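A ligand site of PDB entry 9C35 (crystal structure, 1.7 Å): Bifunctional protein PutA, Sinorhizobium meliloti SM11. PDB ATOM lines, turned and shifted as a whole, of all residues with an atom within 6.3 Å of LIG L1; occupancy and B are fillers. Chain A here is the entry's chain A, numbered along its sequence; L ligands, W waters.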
ATOM      1  N   GLU A 676     -16.668   8.419  14.956  1.00  0.00           N
ATOM      2  CA  GLU A 676     -16.776   9.241  16.176  1.00  0.00           C
ATOM      3  C   GLU A 676     -15.688  10.295  16.207  1.00  0.00           C
ATOM      4  O   GLU A 676     -15.871  11.390  16.774  1.00  0.00           O
ATOM      5  CB  GLU A 676     -16.690   8.341  17.412  1.00  0.00           C
ATOM      6  CG  GLU A 676     -16.953   9.110  18.729  1.00  0.00           C
ATOM      7  CD  GLU A 676     -17.323   8.197  19.891  1.00  0.00           C
ATOM      8  OE1 GLU A 676     -18.333   7.443  19.769  1.00  0.00           O
ATOM      9  OE2 GLU A 676     -16.620   8.218  20.915  1.00  0.00           O
ATOM     10  N   ASN A 709      -8.585   2.441  24.963  1.00  0.00           N
ATOM     11  CA  ASN A 709      -9.728   1.671  24.453  1.00  0.00           C
ATOM     12  C   ASN A 709     -10.565   2.413  23.418  1.00  0.00           C
ATOM     13  O   ASN A 709     -11.362   1.790  22.721  1.00  0.00           O
ATOM     14  CB  ASN A 709     -10.642   1.259  25.618  1.00  0.00           C
ATOM     15  CG  ASN A 709     -11.451   2.419  26.162  1.00  0.00           C
ATOM     16  OD1 ASN A 709     -10.908   3.431  26.567  1.00  0.00           O
ATOM     17  ND2 ASN A 709     -12.772   2.267  26.133  1.00  0.00           N
ATOM     18  N   PHE A 710     -10.399   3.725  23.310  1.00  0.00           N
ATOM     19  CA  PHE A 710     -10.873   4.494  22.164  1.00  0.00           C
ATOM     20  C   PHE A 710      -9.673   5.312  21.715  1.00  0.00           C
ATOM     21  O   PHE A 710      -9.609   6.528  21.936  1.00  0.00           O
ATOM     22  CB  PHE A 710     -12.092   5.355  22.498  1.00  0.00           C
ATOM     23  CG  PHE A 710     -13.332   4.534  22.675  1.00  0.00           C
ATOM     24  CD1 PHE A 710     -14.035   4.093  21.586  1.00  0.00           C
ATOM     25  CD2 PHE A 710     -13.785   4.171  23.941  1.00  0.00           C
ATOM     26  CE1 PHE A 710     -15.165   3.310  21.728  1.00  0.00           C
ATOM     27  CE2 PHE A 710     -14.916   3.388  24.083  1.00  0.00           C
ATOM     28  CZ  PHE A 710     -15.594   2.955  22.969  1.00  0.00           C
ATOM     29  N   ILE A 714     -11.511   9.276  21.406  1.00  0.00           N
ATOM     30  CA  ILE A 714     -11.412  10.135  22.578  1.00  0.00           C
ATOM     31  C   ILE A 714     -10.131  10.967  22.491  1.00  0.00           C
ATOM     32  O   ILE A 714     -10.135  12.164  22.821  1.00  0.00           O
ATOM     33  CB  ILE A 714     -11.482   9.297  23.867  1.00  0.00           C
ATOM     34  CG1 ILE A 714     -12.936   8.799  24.036  1.00  0.00           C
ATOM     35  CG2 ILE A 714     -11.025  10.110  25.092  1.00  0.00           C
ATOM     36  CD1 ILE A 714     -13.140   7.755  25.084  1.00  0.00           C
ATOM     37  N   THR A 783      -8.992  11.366  30.307  1.00  0.00           N
ATOM     38  CA  THR A 783      -9.958  10.263  30.243  1.00  0.00           C
ATOM     39  C   THR A 783      -9.183   8.993  30.570  1.00  0.00           C
ATOM     40  O   THR A 783      -8.131   8.748  29.981  1.00  0.00           O
ATOM     41  CB  THR A 783     -10.614  10.197  28.850  1.00  0.00           C
ATOM     42  OG1 THR A 783     -11.264  11.449  28.569  1.00  0.00           O
ATOM     43  CG2 THR A 783     -11.642   9.034  28.812  1.00  0.00           C
ATOM     44  N   GLN A 844     -14.515  -3.779  27.006  1.00  0.00           N
ATOM     45  CA  GLN A 844     -13.572  -2.700  27.269  1.00  0.00           C
ATOM     46  C   GLN A 844     -14.118  -1.361  26.779  1.00  0.00           C
ATOM     47  O   GLN A 844     -13.453  -0.621  26.055  1.00  0.00           O
ATOM     48  CB  GLN A 844     -12.237  -3.049  26.628  1.00  0.00           C
ATOM     49  CG  GLN A 844     -11.563  -4.217  27.295  1.00  0.00           C
ATOM     50  CD  GLN A 844     -10.484  -4.805  26.431  1.00  0.00           C
ATOM     51  OE1 GLN A 844      -9.334  -4.967  26.849  1.00  0.00           O
ATOM     52  NE2 GLN A 844     -10.832  -5.104  25.196  1.00  0.00           N
ATOM     53  N   ARG A 845     -15.329  -1.046  27.187  1.00  0.00           N
ATOM     54  CA  ARG A 845     -15.936   0.259  26.993  1.00  0.00           C
ATOM     55  C   ARG A 845     -16.251   0.806  28.365  1.00  0.00           C
ATOM     56  O   ARG A 845     -16.782   0.091  29.220  1.00  0.00           O
ATOM     57  CB  ARG A 845     -17.232   0.199  26.166  1.00  0.00           C
ATOM     58  CG  ARG A 845     -17.106  -0.175  24.709  1.00  0.00           C
ATOM     59  CD  ARG A 845     -18.511  -0.159  24.075  1.00  0.00           C
ATOM     60  NE  ARG A 845     -18.477  -0.492  22.665  1.00  0.00           N
ATOM     61  CZ  ARG A 845     -18.494   0.385  21.677  1.00  0.00           C
ATOM     62  NH1 ARG A 845     -18.553   1.690  21.916  1.00  0.00           N
ATOM     63  NH2 ARG A 845     -18.467  -0.040  20.418  1.00  0.00           N
ATOM     64  N   CYS A 846     -15.945   2.082  28.608  1.00  0.00           N
ATOM     65  CA  CYS A 846     -16.368   2.637  29.883  1.00  0.00           C
ATOM     66  C   CYS A 846     -17.887   2.520  30.053  1.00  0.00           C
ATOM     67  O   CYS A 846     -18.363   2.467  31.180  1.00  0.00           O
ATOM     68  CB  CYS A 846     -15.912   4.094  30.000  1.00  0.00           C
ATOM     69  SG  CYS A 846     -16.492   5.098  28.660  1.00  0.00           S
ATOM     70  N   SER A 847     -18.626   2.476  28.961  1.00  0.00           N
ATOM     71  CA  SER A 847     -20.076   2.407  28.989  1.00  0.00           C
ATOM     72  C   SER A 847     -20.621   0.982  29.114  1.00  0.00           C
ATOM     73  O   SER A 847     -21.838   0.822  29.207  1.00  0.00           O
ATOM     74  CB  SER A 847     -20.634   3.007  27.703  1.00  0.00           C
ATOM     75  OG  SER A 847     -19.982   2.442  26.570  1.00  0.00           O
ATOM     76  N   PHE A 944     -12.793  -4.211  34.048  1.00  0.00           N
ATOM     77  CA  PHE A 944     -12.747  -3.698  32.681  1.00  0.00           C
ATOM     78  C   PHE A 944     -12.483  -4.852  31.725  1.00  0.00           C
ATOM     79  O   PHE A 944     -11.390  -5.027  31.186  1.00  0.00           O
ATOM     80  CB  PHE A 944     -11.697  -2.587  32.549  1.00  0.00           C
ATOM     81  CG  PHE A 944     -12.024  -1.583  31.463  1.00  0.00           C
ATOM     82  CD1 PHE A 944     -13.130  -0.751  31.584  1.00  0.00           C
ATOM     83  CD2 PHE A 944     -11.231  -1.466  30.337  1.00  0.00           C
ATOM     84  CE1 PHE A 944     -13.424   0.154  30.590  1.00  0.00           C
ATOM     85  CE2 PHE A 944     -11.527  -0.532  29.334  1.00  0.00           C
ATOM     86  CZ  PHE A 944     -12.630   0.259  29.472  1.00  0.00           C
ATOM     87  N   LEU A 972     -22.311   6.695  35.102  1.00  0.00           N
ATOM     88  CA  LEU A 972     -22.024   6.912  33.696  1.00  0.00           C
ATOM     89  C   LEU A 972     -23.200   6.506  32.807  1.00  0.00           C
ATOM     90  O   LEU A 972     -24.017   7.381  32.436  1.00  0.00           O
ATOM     91  CB  LEU A 972     -20.746   6.175  33.302  1.00  0.00           C
ATOM     92  CG  LEU A 972     -20.145   6.381  31.924  1.00  0.00           C
ATOM     93  CD1 LEU A 972     -19.962   7.838  31.568  1.00  0.00           C
ATOM     94  CD2 LEU A 972     -18.774   5.705  31.825  1.00  0.00           C
ATOM     95  N   THR A 973     -23.285   5.239  32.415  1.00  0.00           N
ATOM     96  CA  THR A 973     -24.407   4.788  31.585  1.00  0.00           C
ATOM     97  C   THR A 973     -25.390   3.932  32.394  1.00  0.00           C
ATOM     98  O   THR A 973     -25.010   3.312  33.385  1.00  0.00           O
ATOM     99  CB  THR A 973     -23.956   3.986  30.329  1.00  0.00           C
ATOM    100  OG1 THR A 973     -23.134   2.874  30.683  1.00  0.00           O
ATOM    101  CG2 THR A 973     -23.147   4.871  29.416  1.00  0.00           C
ATOM    102  N   TYR A 997     -30.620   5.120  28.678  1.00  0.00           N
ATOM    103  CA  TYR A 997     -30.993   4.434  27.460  1.00  0.00           C
ATOM    104  C   TYR A 997     -32.238   3.609  27.753  1.00  0.00           C
ATOM    105  O   TYR A 997     -32.198   2.751  28.633  1.00  0.00           O
ATOM    106  CB  TYR A 997     -29.847   3.539  26.943  1.00  0.00           C
ATOM    107  CG  TYR A 997     -28.570   4.310  26.635  1.00  0.00           C
ATOM    108  CD1 TYR A 997     -28.449   5.004  25.449  1.00  0.00           C
ATOM    109  CD2 TYR A 997     -27.509   4.347  27.542  1.00  0.00           C
ATOM    110  CE1 TYR A 997     -27.287   5.738  25.162  1.00  0.00           C
ATOM    111  CE2 TYR A 997     -26.358   5.061  27.253  1.00  0.00           C
ATOM    112  CZ  TYR A 997     -26.260   5.729  26.054  1.00  0.00           C
ATOM    113  OH  TYR A 997     -25.131   6.458  25.749  1.00  0.00           O
ATOM    114  N   ILE A1002     -26.723   0.210  25.652  1.00  0.00           N
ATOM    115  CA  ILE A1002     -26.246   1.358  26.420  1.00  0.00           C
ATOM    116  C   ILE A1002     -24.873   1.848  25.935  1.00  0.00           C
ATOM    117  O   ILE A1002     -24.210   2.611  26.673  1.00  0.00           O
ATOM    118  CB  ILE A1002     -26.216   1.071  27.934  1.00  0.00           C
ATOM    119  CG1 ILE A1002     -25.157   0.030  28.325  1.00  0.00           C
ATOM    120  CG2 ILE A1002     -27.611   0.730  28.433  1.00  0.00           C
ATOM    121  CD1 ILE A1002     -25.005  -0.154  29.811  1.00  0.00           C
ATOM    122  N   ILE A1003     -24.442   1.464  24.729  1.00  0.00           N
ATOM    123  CA  ILE A1003     -23.118   1.813  24.217  1.00  0.00           C
ATOM    124  C   ILE A1003     -23.235   2.609  22.909  1.00  0.00           C
ATOM    125  O   ILE A1003     -24.285   2.641  22.257  1.00  0.00           O
ATOM    126  CB  ILE A1003     -22.214   0.582  24.012  1.00  0.00           C
ATOM    127  CG1 ILE A1003     -22.720  -0.248  22.836  1.00  0.00           C
ATOM    128  CG2 ILE A1003     -22.127  -0.212  25.287  1.00  0.00           C
ATOM    129  CD1 ILE A1003     -21.768  -1.412  22.346  1.00  0.00           C
ATOM    130  N   GLY A1004     -22.106   3.191  22.507  1.00  0.00           N
ATOM    131  CA  GLY A1004     -22.042   3.853  21.216  1.00  0.00           C
ATOM    132  C   GLY A1004     -22.705   5.212  21.182  1.00  0.00           C
ATOM    133  O   GLY A1004     -23.324   5.586  20.164  1.00  0.00           O
ATOM    134  N   ALA A1005     -22.639   5.967  22.282  1.00  0.00           N
ATOM    135  CA  ALA A1005     -23.148   7.316  22.282  1.00  0.00           C
ATOM    136  C   ALA A1005     -22.637   8.071  21.056  1.00  0.00           C
ATOM    137  O   ALA A1005     -21.480   7.935  20.656  1.00  0.00           O
ATOM    138  CB  ALA A1005     -22.702   8.041  23.555  1.00  0.00           C
ATOM    139  N   VAL A1006     -23.496   8.909  20.499  1.00  0.00           N
ATOM    140  CA  VAL A1006     -23.255   9.600  19.246  1.00  0.00           C
ATOM    141  C   VAL A1006     -22.979  11.071  19.556  1.00  0.00           C
ATOM    142  O   VAL A1006     -23.782  11.704  20.249  1.00  0.00           O
ATOM    143  CB  VAL A1006     -24.487   9.460  18.317  1.00  0.00           C
ATOM    144  CG1 VAL A1006     -24.394  10.365  17.137  1.00  0.00           C
ATOM    145  CG2 VAL A1006     -24.639   7.997  17.871  1.00  0.00           C
ATOM    146  N   PHE A1012     -21.856  12.777  25.891  1.00  0.00           N
ATOM    147  CA  PHE A1012     -21.417  11.685  26.730  1.00  0.00           C
ATOM    148  C   PHE A1012     -20.629  12.127  27.955  1.00  0.00           C
ATOM    149  O   PHE A1012     -19.649  12.891  27.861  1.00  0.00           O
ATOM    150  CB  PHE A1012     -20.575  10.665  25.932  1.00  0.00           C
ATOM    151  CG  PHE A1012     -20.278   9.432  26.696  1.00  0.00           C
ATOM    152  CD1 PHE A1012     -21.260   8.452  26.841  1.00  0.00           C
ATOM    153  CD2 PHE A1012     -19.072   9.251  27.306  1.00  0.00           C
ATOM    154  CE1 PHE A1012     -21.032   7.338  27.578  1.00  0.00           C
ATOM    155  CE2 PHE A1012     -18.827   8.109  28.054  1.00  0.00           C
ATOM    156  CZ  PHE A1012     -19.824   7.139  28.188  1.00  0.00           C
HETATM  157  N1  LIG L   1     -18.572   6.848  24.589  1.00  0.00           N
HETATM  158  C1  LIG L   1     -18.314   5.474  24.214  1.00  0.00           C
HETATM  159  C2  LIG L   1     -19.592   4.645  24.111  1.00  0.00           C
HETATM  160  C3  LIG L   1     -17.572   4.745  25.328  1.00  0.00           C
HETATM  161  C4  LIG L   1     -16.432   5.607  25.871  1.00  0.00           C
HETATM  162  C5  LIG L   1     -15.887   4.807  27.046  1.00  0.00           C
HETATM  163  O1  LIG L   1     -15.083   3.914  26.963  1.00  0.00           O
HETATM  164  O2  LIG L   1     -20.656   5.211  24.444  1.00  0.00           O
HETATM  165  O3  LIG L   1     -19.560   3.446  23.741  1.00  0.00           O
HETATM  166  P1  LG2 L   2      -5.606   4.490  32.824  1.00  0.00           P
HETATM  167  O1  LG2 L   2      -6.090   5.299  34.054  1.00  0.00           O
HETATM  168  O2  LG2 L   2      -4.894   3.252  33.111  1.00  0.00           O
HETATM  169  O3  LG2 L   2      -4.619   5.153  31.926  1.00  0.00           O
HETATM  170  C1  LG2 L   2      -5.020   6.328  31.264  1.00  0.00           C
HETATM  171  C2  LG2 L   2      -3.965   7.337  30.842  1.00  0.00           C
HETATM  172  O4  LG2 L   2      -3.355   8.051  31.927  1.00  0.00           O
HETATM  173  C3  LG2 L   2      -2.818   6.810  30.002  1.00  0.00           C
HETATM  174  O5  LG2 L   2      -2.500   7.706  28.988  1.00  0.00           O
HETATM  175  C4  LG2 L   2      -1.722   6.625  30.999  1.00  0.00           C
HETATM  176  O6  LG2 L   2      -0.518   6.597  30.335  1.00  0.00           O
HETATM  177  C5  LG2 L   2      -1.951   7.794  31.866  1.00  0.00           C
HETATM  178  N1  LG2 L   2      -1.499   7.694  33.222  1.00  0.00           N
HETATM  179  C6  LG2 L   2      -1.345   6.600  34.037  1.00  0.00           C
HETATM  180  N2  LG2 L   2      -0.898   6.986  35.224  1.00  0.00           N
HETATM  181  C7  LG2 L   2      -0.753   8.355  35.233  1.00  0.00           C
HETATM  182  C8  LG2 L   2      -0.338   9.287  36.150  1.00  0.00           C
HETATM  183  N3  LG2 L   2       0.067   8.924  37.479  1.00  0.00           N
HETATM  184  N4  LG2 L   2      -0.321  10.571  35.796  1.00  0.00           N
HETATM  185  C9  LG2 L   2      -0.695  11.009  34.573  1.00  0.00           C
HETATM  186  N5  LG2 L   2      -1.108  10.130  33.644  1.00  0.00           N
HETATM  187  C10 LG2 L   2      -1.137   8.826  33.958  1.00  0.00           C
HETATM  188  O7  LG2 L   2      -6.734   4.084  31.910  1.00  0.00           O
HETATM  189  P2  LG2 L   2      -6.864   3.040  30.722  1.00  0.00           P
HETATM  190  O8  LG2 L   2      -6.507   1.696  31.304  1.00  0.00           O
HETATM  191  O9  LG2 L   2      -6.083   3.481  29.514  1.00  0.00           O
HETATM  192  O10 LG2 L   2      -8.369   3.051  30.253  1.00  0.00           O
HETATM  193  C11 LG2 L   2      -9.361   2.403  31.001  1.00  0.00           C
HETATM  194  C12 LG2 L   2     -10.131   3.317  31.967  1.00  0.00           C
HETATM  195  O11 LG2 L   2     -10.551   4.519  31.356  1.00  0.00           O
HETATM  196  C13 LG2 L   2     -11.339   2.604  32.504  1.00  0.00           C
HETATM  197  O12 LG2 L   2     -11.516   2.790  33.854  1.00  0.00           O
HETATM  198  C14 LG2 L   2     -12.424   3.212  31.711  1.00  0.00           C
HETATM  199  O13 LG2 L   2     -13.662   3.118  32.289  1.00  0.00           O
HETATM  200  C15 LG2 L   2     -11.938   4.623  31.555  1.00  0.00           C
HETATM  201  N6  LG2 L   2     -12.593   5.282  30.451  1.00  0.00           N
HETATM  202  C16 LG2 L   2     -13.556   6.303  30.690  1.00  0.00           C
HETATM  203  C17 LG2 L   2     -14.167   6.927  29.610  1.00  0.00           C
HETATM  204  C18 LG2 L   2     -15.170   8.017  29.776  1.00  0.00           C
HETATM  205  O14 LG2 L   2     -15.529   8.658  28.777  1.00  0.00           O
HETATM  206  N7  LG2 L   2     -15.717   8.358  31.057  1.00  0.00           N
HETATM  207  C19 LG2 L   2     -13.848   6.515  28.281  1.00  0.00           C
HETATM  208  C20 LG2 L   2     -12.905   5.499  28.072  1.00  0.00           C
HETATM  209  C21 LG2 L   2     -12.280   4.887  29.147  1.00  0.00           C
HETATM  210  O   HOH W   1     -23.212   4.933  26.133  1.00  0.00           O
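An oxygen (O3) of LIG L1 lies within hydrogen-bond range of the side-chain hydroxyl (OG) of Ser 847 (3.0 Å). The side-chain amide nitrogen (ND2) of Asn 709 lies within hydrogen-bond range of an oxygen (O1) of LIG L1 (3.0 Å). N of Ala 1005 is in hydrogen-bond range of O2 of LIG L1, 3.0 Å away. C5 of LIG L1 is covalently linked to SG of Cys 846. The guanidinium group (NH1) of Arg 845 is in salt-bridge range of an oxygen (O3) of LIG L1, 2.7 Å away. The backbone NH of Cys 846 lies within hydrogen-bond range of an oxygen (O1) of LIG L1 (2.6 Å). N of Gly 1004 sits at hydrogen-bond distance from O3 of LIG L1 (2.8 Å).
OG1 of Thr 973 is in hydrogen-bond range of O of Ser 847, 2.8 Å away. ND2 of Asn 709 lies within hydrogen-bond range of O of Gln 844.
CE2 of Phe 710 touches O1 of LIG L1 (2.9 Å). Ile 1003 touches LIG L1. CD2 of Phe 1012 touches N1 of LIG L1, at 3.7 Å. Hydrophobic or aromatic side chains that line LIG L1: Phe 710, Ile 1003, Ala 1005 and Phe 1012. Of the 19 residues printed, 9 come within 4 Å of LIG L1.
Water W1 lies within hydrogen-bond range of OH of Tyr 997, O of Ile 1002 and O2 of LIG L1.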
